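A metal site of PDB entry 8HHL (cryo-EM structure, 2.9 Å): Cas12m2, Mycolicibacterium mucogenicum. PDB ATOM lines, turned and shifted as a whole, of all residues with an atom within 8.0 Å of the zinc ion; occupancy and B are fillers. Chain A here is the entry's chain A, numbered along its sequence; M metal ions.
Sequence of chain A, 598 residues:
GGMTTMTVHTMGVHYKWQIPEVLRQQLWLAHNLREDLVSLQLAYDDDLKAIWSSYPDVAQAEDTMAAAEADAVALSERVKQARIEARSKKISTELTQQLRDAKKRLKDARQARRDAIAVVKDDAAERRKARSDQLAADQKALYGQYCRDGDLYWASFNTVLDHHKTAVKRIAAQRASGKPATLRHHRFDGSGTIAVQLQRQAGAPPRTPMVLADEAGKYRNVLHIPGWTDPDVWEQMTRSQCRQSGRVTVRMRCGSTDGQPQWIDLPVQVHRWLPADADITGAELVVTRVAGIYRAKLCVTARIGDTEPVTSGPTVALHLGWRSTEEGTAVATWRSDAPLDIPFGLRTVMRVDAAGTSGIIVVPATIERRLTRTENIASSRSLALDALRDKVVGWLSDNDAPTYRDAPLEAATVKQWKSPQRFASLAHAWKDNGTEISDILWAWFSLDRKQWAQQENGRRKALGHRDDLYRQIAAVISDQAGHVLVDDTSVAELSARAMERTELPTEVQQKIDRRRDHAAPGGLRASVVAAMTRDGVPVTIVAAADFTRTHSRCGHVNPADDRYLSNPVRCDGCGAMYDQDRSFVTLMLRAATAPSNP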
ATOM      1  N   ARG A 549      -5.980  -5.583  12.721  1.00  0.00           N
ATOM      2  CA  ARG A 549      -6.283  -6.991  12.866  1.00  0.00           C
ATOM      3  C   ARG A 549      -5.549  -7.849  11.848  1.00  0.00           C
ATOM      4  O   ARG A 549      -5.682  -9.074  11.881  1.00  0.00           O
ATOM      5  CB  ARG A 549      -7.787  -7.231  12.733  1.00  0.00           C
ATOM      6  CG  ARG A 549      -8.646  -6.189  13.428  1.00  0.00           C
ATOM      7  CD  ARG A 549      -9.875  -6.814  14.037  1.00  0.00           C
ATOM      8  NE  ARG A 549     -10.350  -7.960  13.260  1.00  0.00           N
ATOM      9  CZ  ARG A 549     -11.372  -7.909  12.417  1.00  0.00           C
ATOM     10  NH1 ARG A 549     -12.058  -6.797  12.222  1.00  0.00           N
ATOM     11  NH2 ARG A 549     -11.717  -9.012  11.744  1.00  0.00           N
ATOM     12  N   THR A 550      -4.787  -7.239  10.949  1.00  0.00           N
ATOM     13  CA  THR A 550      -4.036  -7.955   9.924  1.00  0.00           C
ATOM     14  C   THR A 550      -2.551  -7.923  10.268  1.00  0.00           C
ATOM     15  O   THR A 550      -2.013  -6.853  10.572  1.00  0.00           O
ATOM     16  CB  THR A 550      -4.273  -7.336   8.547  1.00  0.00           C
ATOM     17  OG1 THR A 550      -5.676  -7.313   8.259  1.00  0.00           O
ATOM     18  CG2 THR A 550      -3.562  -8.147   7.480  1.00  0.00           C
ATOM     19  N   HIS A 551      -1.913  -9.077  10.223  1.00  0.00           N
ATOM     20  CA  HIS A 551      -0.479  -9.180  10.439  1.00  0.00           C
ATOM     21  C   HIS A 551       0.226  -9.013   9.103  1.00  0.00           C
ATOM     22  O   HIS A 551      -0.092  -9.720   8.128  1.00  0.00           O
ATOM     23  CB  HIS A 551      -0.115 -10.510  11.081  1.00  0.00           C
ATOM     24  CG  HIS A 551       1.310 -10.607  11.508  1.00  0.00           C
ATOM     25  ND1 HIS A 551       1.964 -11.815  11.667  1.00  0.00           N
ATOM     26  CD2 HIS A 551       2.220  -9.656  11.813  1.00  0.00           C
ATOM     27  CE1 HIS A 551       3.208 -11.600  12.042  1.00  0.00           C
ATOM     28  NE2 HIS A 551       3.392 -10.302  12.143  1.00  0.00           N
ATOM     29  N   SER A 552       1.168  -8.075   9.033  1.00  0.00           N
ATOM     30  CA  SER A 552       1.826  -7.767   7.768  1.00  0.00           C
ATOM     31  C   SER A 552       2.653  -8.950   7.265  1.00  0.00           C
ATOM     32  O   SER A 552       2.616  -9.262   6.070  1.00  0.00           O
ATOM     33  CB  SER A 552       2.707  -6.537   7.918  1.00  0.00           C
ATOM     34  OG  SER A 552       1.922  -5.384   8.176  1.00  0.00           O
ATOM     35  N   ARG A 553       3.388  -9.606   8.160  1.00  0.00           N
ATOM     36  CA  ARG A 553       4.306 -10.666   7.732  1.00  0.00           C
ATOM     37  C   ARG A 553       3.561 -11.851   7.120  1.00  0.00           C
ATOM     38  O   ARG A 553       3.997 -12.397   6.097  1.00  0.00           O
ATOM     39  CB  ARG A 553       5.171 -11.115   8.905  1.00  0.00           C
ATOM     40  CG  ARG A 553       6.191 -12.179   8.547  1.00  0.00           C
ATOM     41  CD  ARG A 553       7.273 -12.286   9.604  1.00  0.00           C
ATOM     42  NE  ARG A 553       8.041 -11.050   9.732  1.00  0.00           N
ATOM     43  CZ  ARG A 553       8.066 -10.287  10.811  1.00  0.00           C
ATOM     44  NH1 ARG A 553       7.385 -10.614  11.900  1.00  0.00           N
ATOM     45  NH2 ARG A 553       8.796  -9.182  10.814  1.00  0.00           N
ATOM     46  N   CYS A 554       2.450 -12.260   7.730  1.00  0.00           N
ATOM     47  CA  CYS A 554       1.736 -13.451   7.277  1.00  0.00           C
ATOM     48  C   CYS A 554       0.464 -13.139   6.510  1.00  0.00           C
ATOM     49  O   CYS A 554      -0.046 -14.022   5.809  1.00  0.00           O
ATOM     50  CB  CYS A 554       1.404 -14.355   8.470  1.00  0.00           C
ATOM     51  SG  CYS A 554       0.070 -13.747   9.523  1.00  0.00           S
ATOM     52  N   GLY A 555      -0.055 -11.928   6.614  1.00  0.00           N
ATOM     53  CA  GLY A 555      -1.275 -11.578   5.900  1.00  0.00           C
ATOM     54  C   GLY A 555      -2.514 -12.317   6.373  1.00  0.00           C
ATOM     55  O   GLY A 555      -3.335 -12.734   5.552  1.00  0.00           O
ATOM     56  N   HIS A 556      -2.664 -12.485   7.684  1.00  0.00           N
ATOM     57  CA  HIS A 556      -3.816 -13.134   8.270  1.00  0.00           C
ATOM     58  C   HIS A 556      -4.591 -12.129   9.108  1.00  0.00           C
ATOM     59  O   HIS A 556      -4.005 -11.241   9.734  1.00  0.00           O
ATOM     60  CB  HIS A 556      -3.411 -14.334   9.134  1.00  0.00           C
ATOM     61  CG  HIS A 556      -4.552 -15.234   9.482  1.00  0.00           C
ATOM     62  ND1 HIS A 556      -5.090 -15.299  10.757  1.00  0.00           N
ATOM     63  CD2 HIS A 556      -5.242 -16.126   8.736  1.00  0.00           C
ATOM     64  CE1 HIS A 556      -6.074 -16.179  10.772  1.00  0.00           C
ATOM     65  NE2 HIS A 556      -6.189 -16.700   9.564  1.00  0.00           N
ATOM     66  N   VAL A 557      -5.919 -12.273   9.130  1.00  0.00           N
ATOM     67  CA  VAL A 557      -6.802 -11.361   9.846  1.00  0.00           C
ATOM     68  C   VAL A 557      -7.166 -12.018  11.172  1.00  0.00           C
ATOM     69  O   VAL A 557      -7.847 -13.052  11.206  1.00  0.00           O
ATOM     70  CB  VAL A 557      -8.030 -11.005   9.012  1.00  0.00           C
ATOM     71  CG1 VAL A 557      -7.655 -10.001   7.942  1.00  0.00           C
ATOM     72  CG2 VAL A 557      -8.631 -12.241   8.366  1.00  0.00           C
ATOM     73  N   ASN A 558      -6.696 -11.432  12.267  1.00  0.00           N
ATOM     74  CA  ASN A 558      -7.003 -11.944  13.604  1.00  0.00           C
ATOM     75  C   ASN A 558      -8.422 -11.526  14.003  1.00  0.00           C
ATOM     76  O   ASN A 558      -8.932 -10.506  13.517  1.00  0.00           O
ATOM     77  CB  ASN A 558      -5.978 -11.422  14.614  1.00  0.00           C
ATOM     78  CG  ASN A 558      -4.565 -11.829  14.260  1.00  0.00           C
ATOM     79  OD1 ASN A 558      -3.620 -11.080  14.481  1.00  0.00           O
ATOM     80  ND2 ASN A 558      -4.420 -13.014  13.689  1.00  0.00           N
ATOM     81  N   VAL A 569       0.750  -7.623  20.064  1.00  0.00           N
ATOM     82  CA  VAL A 569      -0.470  -8.405  19.918  1.00  0.00           C
ATOM     83  C   VAL A 569      -0.125  -9.760  19.339  1.00  0.00           C
ATOM     84  O   VAL A 569       0.656  -9.876  18.378  1.00  0.00           O
ATOM     85  CB  VAL A 569      -1.515  -7.680  19.039  1.00  0.00           C
ATOM     86  CG1 VAL A 569      -2.776  -8.510  18.923  1.00  0.00           C
ATOM     87  CG2 VAL A 569      -1.828  -6.315  19.599  1.00  0.00           C
ATOM     88  N   ARG A 570      -0.711 -10.800  19.913  1.00  0.00           N
ATOM     89  CA  ARG A 570      -0.494 -12.170  19.485  1.00  0.00           C
ATOM     90  C   ARG A 570      -1.316 -12.459  18.230  1.00  0.00           C
ATOM     91  O   ARG A 570      -2.507 -12.136  18.175  1.00  0.00           O
ATOM     92  CB  ARG A 570      -0.876 -13.153  20.590  1.00  0.00           C
ATOM     93  CG  ARG A 570      -0.998 -14.593  20.137  1.00  0.00           C
ATOM     94  CD  ARG A 570       0.372 -15.201  19.878  1.00  0.00           C
ATOM     95  NE  ARG A 570       1.183 -15.265  21.075  1.00  0.00           N
ATOM     96  CZ  ARG A 570       2.438 -15.689  21.121  1.00  0.00           C
ATOM     97  NH1 ARG A 570       3.059 -16.096  20.030  1.00  0.00           N
ATOM     98  NH2 ARG A 570       3.084 -15.706  22.277  1.00  0.00           N
ATOM     99  N   CYS A 571      -0.674 -13.050  17.229  1.00  0.00           N
ATOM    100  CA  CYS A 571      -1.331 -13.414  15.983  1.00  0.00           C
ATOM    101  C   CYS A 571      -1.691 -14.893  15.987  1.00  0.00           C
ATOM    102  O   CYS A 571      -1.040 -15.711  16.635  1.00  0.00           O
ATOM    103  CB  CYS A 571      -0.433 -13.104  14.786  1.00  0.00           C
ATOM    104  SG  CYS A 571      -1.099 -13.670  13.199  1.00  0.00           S
ATOM    105  N   ASP A 572      -2.749 -15.224  15.250  1.00  0.00           N
ATOM    106  CA  ASP A 572      -3.201 -16.608  15.144  1.00  0.00           C
ATOM    107  C   ASP A 572      -2.659 -17.314  13.919  1.00  0.00           C
ATOM    108  O   ASP A 572      -2.413 -18.520  13.956  1.00  0.00           O
ATOM    109  CB  ASP A 572      -4.730 -16.673  15.136  1.00  0.00           C
ATOM    110  CG  ASP A 572      -5.343 -16.076  16.384  1.00  0.00           C
ATOM    111  OD1 ASP A 572      -4.588 -15.678  17.294  1.00  0.00           O
ATOM    112  OD2 ASP A 572      -6.592 -15.993  16.460  1.00  0.00           O
ATOM    113  N   GLY A 573      -2.469 -16.587  12.805  1.00  0.00           N
ATOM    114  CA  GLY A 573      -1.991 -17.216  11.594  1.00  0.00           C
ATOM    115  C   GLY A 573      -0.569 -17.736  11.722  1.00  0.00           C
ATOM    116  O   GLY A 573      -0.259 -18.854  11.308  1.00  0.00           O
ATOM    117  N   CYS A 574       0.322 -16.934  12.314  1.00  0.00           N
ATOM    118  CA  CYS A 574       1.724 -17.293  12.454  1.00  0.00           C
ATOM    119  C   CYS A 574       2.121 -17.598  13.888  1.00  0.00           C
ATOM    120  O   CYS A 574       3.213 -18.134  14.102  1.00  0.00           O
ATOM    121  CB  CYS A 574       2.606 -16.168  11.900  1.00  0.00           C
ATOM    122  SG  CYS A 574       2.351 -14.551  12.665  1.00  0.00           S
ATOM    123  N   GLY A 575       1.274 -17.301  14.863  1.00  0.00           N
ATOM    124  CA  GLY A 575       1.617 -17.578  16.245  1.00  0.00           C
ATOM    125  C   GLY A 575       2.791 -16.764  16.757  1.00  0.00           C
ATOM    126  O   GLY A 575       3.651 -17.299  17.470  1.00  0.00           O
ATOM    127  N   ALA A 576       2.841 -15.486  16.404  1.00  0.00           N
ATOM    128  CA  ALA A 576       3.910 -14.602  16.845  1.00  0.00           C
ATOM    129  C   ALA A 576       3.321 -13.269  17.271  1.00  0.00           C
ATOM    130  O   ALA A 576       2.249 -12.859  16.795  1.00  0.00           O
ATOM    131  CB  ALA A 576       4.971 -14.397  15.763  1.00  0.00           C
ATOM    132  N   MET A 577       4.029 -12.586  18.166  1.00  0.00           N
ATOM    133  CA  MET A 577       3.585 -11.294  18.674  1.00  0.00           C
ATOM    134  C   MET A 577       4.108 -10.185  17.764  1.00  0.00           C
ATOM    135  O   MET A 577       5.301 -10.125  17.475  1.00  0.00           O
ATOM    136  CB  MET A 577       4.091 -11.085  20.102  1.00  0.00           C
ATOM    137  CG  MET A 577       3.542 -12.099  21.102  1.00  0.00           C
ATOM    138  SD  MET A 577       3.555 -11.484  22.790  1.00  0.00           S
ATOM    139  CE  MET A 577       2.380 -10.136  22.674  1.00  0.00           C
ATOM    140  N   TYR A 578       3.202  -9.322  17.318  1.00  0.00           N
ATOM    141  CA  TYR A 578       3.527  -8.249  16.388  1.00  0.00           C
ATOM    142  C   TYR A 578       3.027  -6.916  16.902  1.00  0.00           C
ATOM    143  O   TYR A 578       1.961  -6.841  17.538  1.00  0.00           O
ATOM    144  CB  TYR A 578       2.946  -8.530  15.005  1.00  0.00           C
ATOM    145  CG  TYR A 578       1.435  -8.467  14.932  1.00  0.00           C
ATOM    146  CD1 TYR A 578       0.665  -9.583  15.206  1.00  0.00           C
ATOM    147  CD2 TYR A 578       0.785  -7.296  14.571  1.00  0.00           C
ATOM    148  CE1 TYR A 578      -0.712  -9.533  15.144  1.00  0.00           C
ATOM    149  CE2 TYR A 578      -0.594  -7.236  14.500  1.00  0.00           C
ATOM    150  CZ  TYR A 578      -1.338  -8.365  14.784  1.00  0.00           C
ATOM    151  OH  TYR A 578      -2.710  -8.307  14.719  1.00  0.00           O
HETATM  152 ZN    ZN M   1       0.659 -13.377  11.709  1.00  0.00          ZN
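ND2 of Asn 558 lies close to SG of Cys 571 (3.4 Å). The backbone NH (N) of Cys 571 is in hydrogen-bond range of the backbone carbonyl oxygen (O) of Ala 576 (3.0 Å). The backbone NH (N) of His 556 sits close to the side-chain sulfur (SG) of Cys 554 (3.5 Å). The backbone NH (N) of His 551 is in hydrogen-bond range of the backbone carbonyl oxygen (O) of His 556, at 3.0 Å. The side-chain sulfur (SG) of Cys 571 sits close to the backbone NH (N) of Gly 573, 3.2 Å away.
The nearest printed residue that does not touch the zinc ion is Gly 573 (4.5 Å).
The zinc ion is bound by ND1 of His 551 (2.0 Å), SG of Cys 574 (2.3 Å), SG of Cys 554 (2.3 Å) and SG of Cys 571 (2.3 Å).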
